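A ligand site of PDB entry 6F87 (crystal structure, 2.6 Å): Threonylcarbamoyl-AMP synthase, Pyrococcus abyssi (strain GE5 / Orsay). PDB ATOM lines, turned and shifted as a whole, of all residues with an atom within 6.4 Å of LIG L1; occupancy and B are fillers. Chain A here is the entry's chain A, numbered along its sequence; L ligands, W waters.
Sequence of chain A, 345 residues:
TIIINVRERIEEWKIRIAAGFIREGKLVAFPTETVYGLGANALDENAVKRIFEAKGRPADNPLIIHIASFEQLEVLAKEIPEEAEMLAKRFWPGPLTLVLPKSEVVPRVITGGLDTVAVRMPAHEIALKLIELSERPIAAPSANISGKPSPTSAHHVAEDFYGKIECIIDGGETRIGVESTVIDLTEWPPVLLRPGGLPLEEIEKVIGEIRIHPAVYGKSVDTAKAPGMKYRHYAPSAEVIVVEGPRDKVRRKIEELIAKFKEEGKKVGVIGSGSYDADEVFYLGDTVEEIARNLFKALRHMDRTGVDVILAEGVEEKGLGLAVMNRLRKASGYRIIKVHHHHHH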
ATOM      1  N   LYS A  55       7.626 -14.661   7.326  1.00  0.00           N
ATOM      2  CA  LYS A  55       7.614 -15.935   8.003  1.00  0.00           C
ATOM      3  C   LYS A  55       6.375 -16.787   7.684  1.00  0.00           C
ATOM      4  O   LYS A  55       6.387 -18.046   7.801  1.00  0.00           O
ATOM      5  CB  LYS A  55       7.642 -15.673   9.496  1.00  0.00           C
ATOM      6  CG  LYS A  55       8.950 -15.089  10.034  1.00  0.00           C
ATOM      7  CD  LYS A  55       9.031 -15.183  11.546  1.00  0.00           C
ATOM      8  CE  LYS A  55       8.942 -16.614  11.992  1.00  0.00           C
ATOM      9  NZ  LYS A  55       9.865 -16.927  13.074  1.00  0.00           N
ATOM     10  N   GLY A  56       5.297 -16.110   7.337  1.00  0.00           N
ATOM     11  CA  GLY A  56       3.993 -16.787   7.308  1.00  0.00           C
ATOM     12  C   GLY A  56       3.485 -17.005   8.722  1.00  0.00           C
ATOM     13  O   GLY A  56       2.909 -18.036   9.037  1.00  0.00           O
ATOM     14  N   ARG A  57       3.680 -16.001   9.567  1.00  0.00           N
ATOM     15  CA  ARG A  57       3.336 -16.057  10.962  1.00  0.00           C
ATOM     16  C   ARG A  57       1.900 -15.540  11.194  1.00  0.00           C
ATOM     17  O   ARG A  57       1.597 -14.399  10.844  1.00  0.00           O
ATOM     18  CB  ARG A  57       4.305 -15.182  11.766  1.00  0.00           C
ATOM     19  CG  ARG A  57       4.221 -15.436  13.258  1.00  0.00           C
ATOM     20  CD  ARG A  57       5.081 -14.456  13.948  1.00  0.00           C
ATOM     21  NE  ARG A  57       5.177 -14.648  15.390  1.00  0.00           N
ATOM     22  CZ  ARG A  57       5.943 -15.549  15.984  1.00  0.00           C
ATOM     23  NH1 ARG A  57       6.620 -16.434  15.254  1.00  0.00           N
ATOM     24  NH2 ARG A  57       6.008 -15.602  17.315  1.00  0.00           N
ATOM     25  N   PRO A  58       1.045 -16.317  11.846  1.00  0.00           N
ATOM     26  CA  PRO A  58      -0.237 -15.858  12.293  1.00  0.00           C
ATOM     27  C   PRO A  58      -0.131 -14.616  13.145  1.00  0.00           C
ATOM     28  O   PRO A  58       0.778 -14.495  13.948  1.00  0.00           O
ATOM     29  CB  PRO A  58      -0.735 -17.018  13.138  1.00  0.00           C
ATOM     30  CG  PRO A  58      -0.120 -18.223  12.545  1.00  0.00           C
ATOM     31  CD  PRO A  58       1.248 -17.759  12.143  1.00  0.00           C
ATOM     32  N   ASN A  61       0.367 -14.445  17.127  1.00  0.00           N
ATOM     33  CA  ASN A  61       1.508 -15.033  17.749  1.00  0.00           C
ATOM     34  C   ASN A  61       2.534 -13.901  17.944  1.00  0.00           C
ATOM     35  O   ASN A  61       3.193 -13.527  16.999  1.00  0.00           O
ATOM     36  CB  ASN A  61       2.051 -16.178  16.914  1.00  0.00           C
ATOM     37  CG  ASN A  61       3.118 -16.978  17.620  1.00  0.00           C
ATOM     38  OD1 ASN A  61       3.392 -16.777  18.779  1.00  0.00           O
ATOM     39  ND2 ASN A  61       3.728 -17.892  16.906  1.00  0.00           N
ATOM     40  N   PRO A  62       2.688 -13.418  19.195  1.00  0.00           N
ATOM     41  CA  PRO A  62       3.494 -12.253  19.490  1.00  0.00           C
ATOM     42  C   PRO A  62       4.981 -12.394  19.262  1.00  0.00           C
ATOM     43  O   PRO A  62       5.501 -13.495  19.145  1.00  0.00           O
ATOM     44  CB  PRO A  62       3.257 -12.006  20.981  1.00  0.00           C
ATOM     45  CG  PRO A  62       2.650 -13.217  21.535  1.00  0.00           C
ATOM     46  CD  PRO A  62       2.379 -14.189  20.426  1.00  0.00           C
ATOM     47  N   LEU A  63       5.645 -11.237  19.299  1.00  0.00           N
ATOM     48  CA  LEU A  63       7.062 -11.096  19.105  1.00  0.00           C
ATOM     49  C   LEU A  63       7.639 -10.524  20.356  1.00  0.00           C
ATOM     50  O   LEU A  63       6.922  -9.882  21.124  1.00  0.00           O
ATOM     51  CB  LEU A  63       7.398 -10.125  17.960  1.00  0.00           C
ATOM     52  CG  LEU A  63       6.634 -10.384  16.671  1.00  0.00           C
ATOM     53  CD1 LEU A  63       7.042  -9.350  15.635  1.00  0.00           C
ATOM     54  CD2 LEU A  63       6.891 -11.796  16.146  1.00  0.00           C
ATOM     55  N   PRO A 141      11.057 -12.445  16.245  1.00  0.00           N
ATOM     56  CA  PRO A 141      11.025 -13.861  16.539  1.00  0.00           C
ATOM     57  C   PRO A 141      12.229 -14.528  15.910  1.00  0.00           C
ATOM     58  O   PRO A 141      13.028 -13.873  15.221  1.00  0.00           O
ATOM     59  CB  PRO A 141       9.749 -14.320  15.848  1.00  0.00           C
ATOM     60  CG  PRO A 141       9.735 -13.490  14.630  1.00  0.00           C
ATOM     61  CD  PRO A 141      10.418 -12.154  14.962  1.00  0.00           C
ATOM     62  N   SER A 142      12.335 -15.836  16.107  1.00  0.00           N
ATOM     63  CA  SER A 142      13.327 -16.678  15.385  1.00  0.00           C
ATOM     64  C   SER A 142      13.340 -16.464  13.833  1.00  0.00           C
ATOM     65  O   SER A 142      12.287 -16.314  13.176  1.00  0.00           O
ATOM     66  CB  SER A 142      13.124 -18.165  15.764  1.00  0.00           C
ATOM     67  OG  SER A 142      11.739 -18.497  15.956  1.00  0.00           O
ATOM     68  N   ALA A 143      14.547 -16.427  13.245  1.00  0.00           N
ATOM     69  CA  ALA A 143      14.703 -16.127  11.805  1.00  0.00           C
ATOM     70  C   ALA A 143      14.555 -17.387  10.892  1.00  0.00           C
ATOM     71  O   ALA A 143      15.491 -17.764  10.179  1.00  0.00           O
ATOM     72  CB  ALA A 143      16.049 -15.422  11.545  1.00  0.00           C
ATOM     73  N   ASN A 144      13.381 -17.998  10.955  1.00  0.00           N
ATOM     74  CA  ASN A 144      13.039 -19.187  10.166  1.00  0.00           C
ATOM     75  C   ASN A 144      11.628 -19.050   9.613  1.00  0.00           C
ATOM     76  O   ASN A 144      10.810 -18.336  10.145  1.00  0.00           O
ATOM     77  CB  ASN A 144      13.074 -20.456  11.015  1.00  0.00           C
ATOM     78  CG  ASN A 144      12.208 -20.361  12.283  1.00  0.00           C
ATOM     79  OD1 ASN A 144      12.568 -19.680  13.219  1.00  0.00           O
ATOM     80  ND2 ASN A 144      11.088 -21.039  12.310  1.00  0.00           N
ATOM     81  N   ILE A 145      11.349 -19.770   8.548  1.00  0.00           N
ATOM     82  CA  ILE A 145       9.965 -19.896   8.065  1.00  0.00           C
ATOM     83  C   ILE A 145       9.128 -20.493   9.173  1.00  0.00           C
ATOM     84  O   ILE A 145       9.602 -21.436   9.803  1.00  0.00           O
ATOM     85  CB  ILE A 145       9.935 -20.822   6.833  1.00  0.00           C
ATOM     86  CG1 ILE A 145      10.309 -20.028   5.594  1.00  0.00           C
ATOM     87  CG2 ILE A 145       8.571 -21.491   6.667  1.00  0.00           C
ATOM     88  CD1 ILE A 145      11.241 -20.823   4.701  1.00  0.00           C
ATOM     89  N   SER A 146       7.895 -19.976   9.384  1.00  0.00           N
ATOM     90  CA  SER A 146       7.023 -20.481  10.501  1.00  0.00           C
ATOM     91  C   SER A 146       6.768 -21.966  10.404  1.00  0.00           C
ATOM     92  O   SER A 146       6.539 -22.500   9.323  1.00  0.00           O
ATOM     93  CB  SER A 146       5.676 -19.771  10.595  1.00  0.00           C
ATOM     94  OG  SER A 146       5.773 -18.554  11.355  1.00  0.00           O
ATOM     95  N   GLY A 147       6.868 -22.626  11.542  1.00  0.00           N
ATOM     96  CA  GLY A 147       6.689 -24.076  11.663  1.00  0.00           C
ATOM     97  C   GLY A 147       7.965 -24.880  11.703  1.00  0.00           C
ATOM     98  O   GLY A 147       7.964 -26.006  12.230  1.00  0.00           O
ATOM     99  N   LYS A 148       9.054 -24.286  11.182  1.00  0.00           N
ATOM    100  CA  LYS A 148      10.303 -25.008  10.874  1.00  0.00           C
ATOM    101  C   LYS A 148      11.340 -24.817  11.948  1.00  0.00           C
ATOM    102  O   LYS A 148      11.198 -23.919  12.779  1.00  0.00           O
ATOM    103  CB  LYS A 148      10.852 -24.597   9.502  1.00  0.00           C
ATOM    104  CG  LYS A 148       9.994 -24.968   8.300  1.00  0.00           C
ATOM    105  CD  LYS A 148       9.390 -26.372   8.351  1.00  0.00           C
ATOM    106  CE  LYS A 148       9.575 -27.215   7.080  1.00  0.00           C
ATOM    107  NZ  LYS A 148       8.968 -28.573   7.305  1.00  0.00           N
ATOM    108  N   SER A 150      14.314 -23.810  14.387  1.00  0.00           N
ATOM    109  CA  SER A 150      14.863 -22.497  14.609  1.00  0.00           C
ATOM    110  C   SER A 150      16.258 -22.431  14.011  1.00  0.00           C
ATOM    111  O   SER A 150      16.897 -23.485  13.821  1.00  0.00           O
ATOM    112  CB  SER A 150      14.808 -22.192  16.087  1.00  0.00           C
ATOM    113  OG  SER A 150      13.479 -22.362  16.510  1.00  0.00           O
ATOM    114  N   GLU A 179      15.953 -21.124  22.473  1.00  0.00           N
ATOM    115  CA  GLU A 179      15.355 -19.805  22.674  1.00  0.00           C
ATOM    116  C   GLU A 179      15.373 -19.402  24.155  1.00  0.00           C
ATOM    117  O   GLU A 179      15.594 -20.227  25.076  1.00  0.00           O
ATOM    118  CB  GLU A 179      13.945 -19.758  22.097  1.00  0.00           C
ATOM    119  CG  GLU A 179      13.840 -19.768  20.584  1.00  0.00           C
ATOM    120  CD  GLU A 179      13.652 -21.146  19.935  1.00  0.00           C
ATOM    121  OE1 GLU A 179      13.994 -22.165  20.572  1.00  0.00           O
ATOM    122  OE2 GLU A 179      13.168 -21.159  18.773  1.00  0.00           O
ATOM    123  N   ARG A 194       7.583 -20.412  28.294  1.00  0.00           N
ATOM    124  CA  ARG A 194       8.415 -21.166  27.407  1.00  0.00           C
ATOM    125  C   ARG A 194       9.749 -21.465  28.073  1.00  0.00           C
ATOM    126  O   ARG A 194      10.451 -20.534  28.454  1.00  0.00           O
ATOM    127  CB  ARG A 194       8.700 -20.386  26.141  1.00  0.00           C
ATOM    128  CG  ARG A 194       9.559 -21.182  25.156  1.00  0.00           C
ATOM    129  CD  ARG A 194       9.725 -20.422  23.866  1.00  0.00           C
ATOM    130  NE  ARG A 194      10.585 -19.262  24.086  1.00  0.00           N
ATOM    131  CZ  ARG A 194      10.870 -18.338  23.187  1.00  0.00           C
ATOM    132  NH1 ARG A 194      10.366 -18.408  21.958  1.00  0.00           N
ATOM    133  NH2 ARG A 194      11.694 -17.347  23.533  1.00  0.00           N
ATOM    134  N   ALA A 226       3.201 -15.188  24.654  1.00  0.00           N
ATOM    135  CA  ALA A 226       4.611 -15.391  24.358  1.00  0.00           C
ATOM    136  C   ALA A 226       4.653 -16.271  23.178  1.00  0.00           C
ATOM    137  O   ALA A 226       3.712 -17.006  22.944  1.00  0.00           O
ATOM    138  CB  ALA A 226       5.307 -16.088  25.522  1.00  0.00           C
ATOM    139  N   PRO A 227       5.763 -16.233  22.469  1.00  0.00           N
ATOM    140  CA  PRO A 227       5.968 -17.153  21.388  1.00  0.00           C
ATOM    141  C   PRO A 227       6.203 -18.561  21.867  1.00  0.00           C
ATOM    142  O   PRO A 227       6.527 -18.788  23.007  1.00  0.00           O
ATOM    143  CB  PRO A 227       7.220 -16.621  20.665  1.00  0.00           C
ATOM    144  CG  PRO A 227       7.824 -15.545  21.507  1.00  0.00           C
ATOM    145  CD  PRO A 227       6.820 -15.203  22.580  1.00  0.00           C
ATOM    146  N   GLY A 228       6.047 -19.507  20.959  1.00  0.00           N
ATOM    147  CA  GLY A 228       6.318 -20.902  21.242  1.00  0.00           C
ATOM    148  C   GLY A 228       5.254 -21.591  22.072  1.00  0.00           C
ATOM    149  O   GLY A 228       5.525 -22.621  22.660  1.00  0.00           O
ATOM    150  N   MET A 229       4.060 -21.023  22.120  1.00  0.00           N
ATOM    151  CA  MET A 229       2.969 -21.598  22.858  1.00  0.00           C
ATOM    152  C   MET A 229       1.874 -22.004  21.908  1.00  0.00           C
ATOM    153  O   MET A 229       1.356 -23.090  22.011  1.00  0.00           O
ATOM    154  CB  MET A 229       2.420 -20.603  23.855  1.00  0.00           C
ATOM    155  CG  MET A 229       3.435 -19.964  24.754  1.00  0.00           C
ATOM    156  SD  MET A 229       2.598 -18.863  25.931  1.00  0.00           S
ATOM    157  CE  MET A 229       1.628 -19.925  26.998  1.00  0.00           C
ATOM    158  N   LYS A 230       1.457 -21.122  21.018  1.00  0.00           N
ATOM    159  CA  LYS A 230       0.429 -21.471  20.063  1.00  0.00           C
ATOM    160  C   LYS A 230       0.977 -21.863  18.670  1.00  0.00           C
ATOM    161  O   LYS A 230       1.959 -21.278  18.191  1.00  0.00           O
ATOM    162  CB  LYS A 230      -0.503 -20.277  19.925  1.00  0.00           C
ATOM    163  CG  LYS A 230      -1.876 -20.650  19.427  1.00  0.00           C
ATOM    164  CD  LYS A 230      -2.695 -19.433  19.101  1.00  0.00           C
ATOM    165  CE  LYS A 230      -4.003 -19.814  18.446  1.00  0.00           C
ATOM    166  NZ  LYS A 230      -4.786 -18.561  18.224  1.00  0.00           N
ATOM    167  N   ARG A 232       2.262 -24.856  15.655  1.00  0.00           N
ATOM    168  CA  ARG A 232       3.282 -25.874  15.706  1.00  0.00           C
ATOM    169  C   ARG A 232       4.598 -25.286  15.339  1.00  0.00           C
ATOM    170  O   ARG A 232       4.674 -24.402  14.504  1.00  0.00           O
ATOM    171  CB  ARG A 232       2.914 -27.067  14.842  1.00  0.00           C
ATOM    172  CG  ARG A 232       2.519 -28.282  15.709  1.00  0.00           C
ATOM    173  CD  ARG A 232       3.734 -29.123  16.122  1.00  0.00           C
ATOM    174  NE  ARG A 232       4.346 -29.763  14.937  1.00  0.00           N
ATOM    175  CZ  ARG A 232       3.842 -30.804  14.251  1.00  0.00           C
ATOM    176  NH1 ARG A 232       2.688 -31.378  14.631  1.00  0.00           N
ATOM    177  NH2 ARG A 232       4.486 -31.270  13.171  1.00  0.00           N
ATOM    178  N   HIS A 233       5.644 -25.772  15.994  1.00  0.00           N
ATOM    179  CA  HIS A 233       6.968 -25.202  15.866  1.00  0.00           C
ATOM    180  C   HIS A 233       8.055 -26.242  15.843  1.00  0.00           C
ATOM    181  O   HIS A 233       7.849 -27.396  16.204  1.00  0.00           O
ATOM    182  CB  HIS A 233       7.244 -24.276  17.030  1.00  0.00           C
ATOM    183  CG  HIS A 233       6.198 -23.264  17.264  1.00  0.00           C
ATOM    184  ND1 HIS A 233       5.969 -22.222  16.385  1.00  0.00           N
ATOM    185  CD2 HIS A 233       5.288 -23.134  18.247  1.00  0.00           C
ATOM    186  CE1 HIS A 233       4.970 -21.487  16.838  1.00  0.00           C
ATOM    187  NE2 HIS A 233       4.532 -22.026  17.969  1.00  0.00           N
ATOM    188  N   TYR A 234       9.243 -25.767  15.461  1.00  0.00           N
ATOM    189  CA  TYR A 234      10.519 -26.491  15.517  1.00  0.00           C
ATOM    190  C   TYR A 234      10.607 -27.735  14.603  1.00  0.00           C
ATOM    191  O   TYR A 234      11.567 -28.508  14.712  1.00  0.00           O
ATOM    192  CB  TYR A 234      10.863 -26.874  16.939  1.00  0.00           C
ATOM    193  CG  TYR A 234      10.568 -25.799  17.927  1.00  0.00           C
ATOM    194  CD1 TYR A 234      11.167 -24.535  17.832  1.00  0.00           C
ATOM    195  CD2 TYR A 234       9.662 -26.018  18.979  1.00  0.00           C
ATOM    196  CE1 TYR A 234      10.878 -23.524  18.765  1.00  0.00           C
ATOM    197  CE2 TYR A 234       9.366 -25.012  19.907  1.00  0.00           C
ATOM    198  CZ  TYR A 234       9.967 -23.759  19.803  1.00  0.00           C
ATOM    199  OH  TYR A 234       9.639 -22.789  20.747  1.00  0.00           O
HETATM  200  P1  LIG L   1       7.658 -18.869  17.348  1.00  0.00           P
HETATM  201  O1  LIG L   1       8.638 -17.665  17.531  1.00  0.00           O
HETATM  202  O2  LIG L   1       8.396 -20.194  17.420  1.00  0.00           O
HETATM  203  O3  LIG L   1       6.418 -18.837  18.178  1.00  0.00           O
HETATM  204  O4  LIG L   1       7.007 -18.876  15.856  1.00  0.00           O
HETATM  205  P2  LIG L   1       7.617 -19.510  14.489  1.00  0.00           P
HETATM  206  O5  LIG L   1       9.103 -19.390  14.663  1.00  0.00           O
HETATM  207  O6  LIG L   1       7.219 -20.978  14.343  1.00  0.00           O
HETATM  208  O7  LIG L   1       7.018 -18.552  13.489  1.00  0.00           O
HETATM  209  N1  LG2 L   2      13.255 -14.633  20.004  1.00  0.00           N
HETATM  210  C1  LG2 L   2      14.537 -15.355  20.264  1.00  0.00           C
HETATM  211  C2  LG2 L   2      14.592 -15.653  21.727  1.00  0.00           C
HETATM  212  O1  LG2 L   2      13.882 -15.112  22.581  1.00  0.00           O
HETATM  213  C3  LG2 L   2      15.828 -14.570  19.904  1.00  0.00           C
HETATM  214  O2  LG2 L   2      15.839 -13.354  20.623  1.00  0.00           O
HETATM  215  C4  LG2 L   2      15.894 -14.256  18.448  1.00  0.00           C
HETATM  216  O3  LG2 L   2      15.386 -16.474  22.089  1.00  0.00           O
HETATM  217  O   HOH W   1       4.331 -19.115  13.950  1.00  0.00           O
HETATM  218  O   HOH W   2       9.020 -22.730  14.710  1.00  0.00           O
HETATM  219  O   HOH W   3      11.046 -21.265  15.962  1.00  0.00           O
HETATM  220  O   HOH W   4       9.718 -20.211  19.911  1.00  0.00           O
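Residues that only touch LIG L1: Pro 141 (3.9 Å) and Pro 227 (3.4 Å). Hydrophobic or aromatic side chains that line LIG L1: Pro 141, Pro 227 and His 233. Within 4 Å of LIG L1: Lys 55, Arg 57, Asn 61, Pro 141, Ser 142, Asn 144, Ser 146, Gly 147, Pro 227, Gly 228 and His 233.
Water W2 lies within hydrogen-bond range of an oxygen (O6) of LIG L1 (2.5 Å), the backbone NH of Tyr 234 (3.1 Å) and the backbone carbonyl oxygen of Lys 148 (3.1 Å). Water W1 lies within hydrogen-bond range of O7 of LIG L1 (2.8 Å), OG of Ser 146 (3.0 Å) and ND2 of Asn 61 (3.3 Å). Water W4 lies within hydrogen-bond range of the side-chain hydroxyl of Tyr 234 (2.7 Å), the guanidinium group of Arg 194 (2.8 Å) and an oxygen (O2) of LIG L1 (2.8 Å). Water W3 lies within hydrogen-bond range of OG of Ser 150 (2.7 Å), OG of Ser 142 (2.9 Å) and O5 of LIG L1 (3.0 Å).
The guanidinium group (NH1) of Arg 57 is in salt-bridge range of an oxygen (O7) of LIG L1 (2.8 Å). The backbone NH (N) of Gly 228 lies within hydrogen-bond range of an oxygen (O3) of LIG L1 (2.9 Å). NH2 of Arg 194 lies within salt-bridge range of O1 of LG2 L2 (3.3 Å). A ring nitrogen (ND1) of His 233 lies within hydrogen-bond range of an oxygen (O6) of LIG L1 (2.7 Å). The side-chain hydroxyl (OG) of Ser 142 is in hydrogen-bond range of an oxygen (O5) of LIG L1 (3.1 Å). An oxygen (O7) of LIG L1 is in hydrogen-bond range of the side-chain hydroxyl (OG) of Ser 146, at 2.5 Å. The side-chain amide nitrogen of Asn 61 sits at hydrogen-bond distance from an oxygen (O3) of LIG L1 (3.1 Å). ND2 of Asn 144 lies within hydrogen-bond range of O5 of LIG L1 (3.5 Å). O5 of LIG L1 lies within salt-bridge range of NZ of Lys 55 (3.0 Å). N of Gly 147 sits at hydrogen-bond distance from O6 of LIG L1 (3.3 Å).
NH2 of Arg 57 is in hydrogen-bond range of O of Pro 62 (2.8 Å). OD1 of Asn 144 lies close to OG of Ser 142 (3.1 Å). N of Ser 146 is in hydrogen-bond range of O of Lys 55 (2.9 Å). The backbone carbonyl oxygen (O) of Gly 147 lies within hydrogen-bond range of the backbone NH (N) of Tyr 234 (3.5 Å). O of Lys 230 is in hydrogen-bond range of NE2 of His 233 (2.7 Å). NZ of Lys 55 is in hydrogen-bond range of O of Ser 142, at 2.5 Å. ND2 of Asn 144 is in hydrogen-bond range of O of Lys 148, 2.9 Å away. NZ of Lys 55 sits close to O of Asn 144 (3.4 Å).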
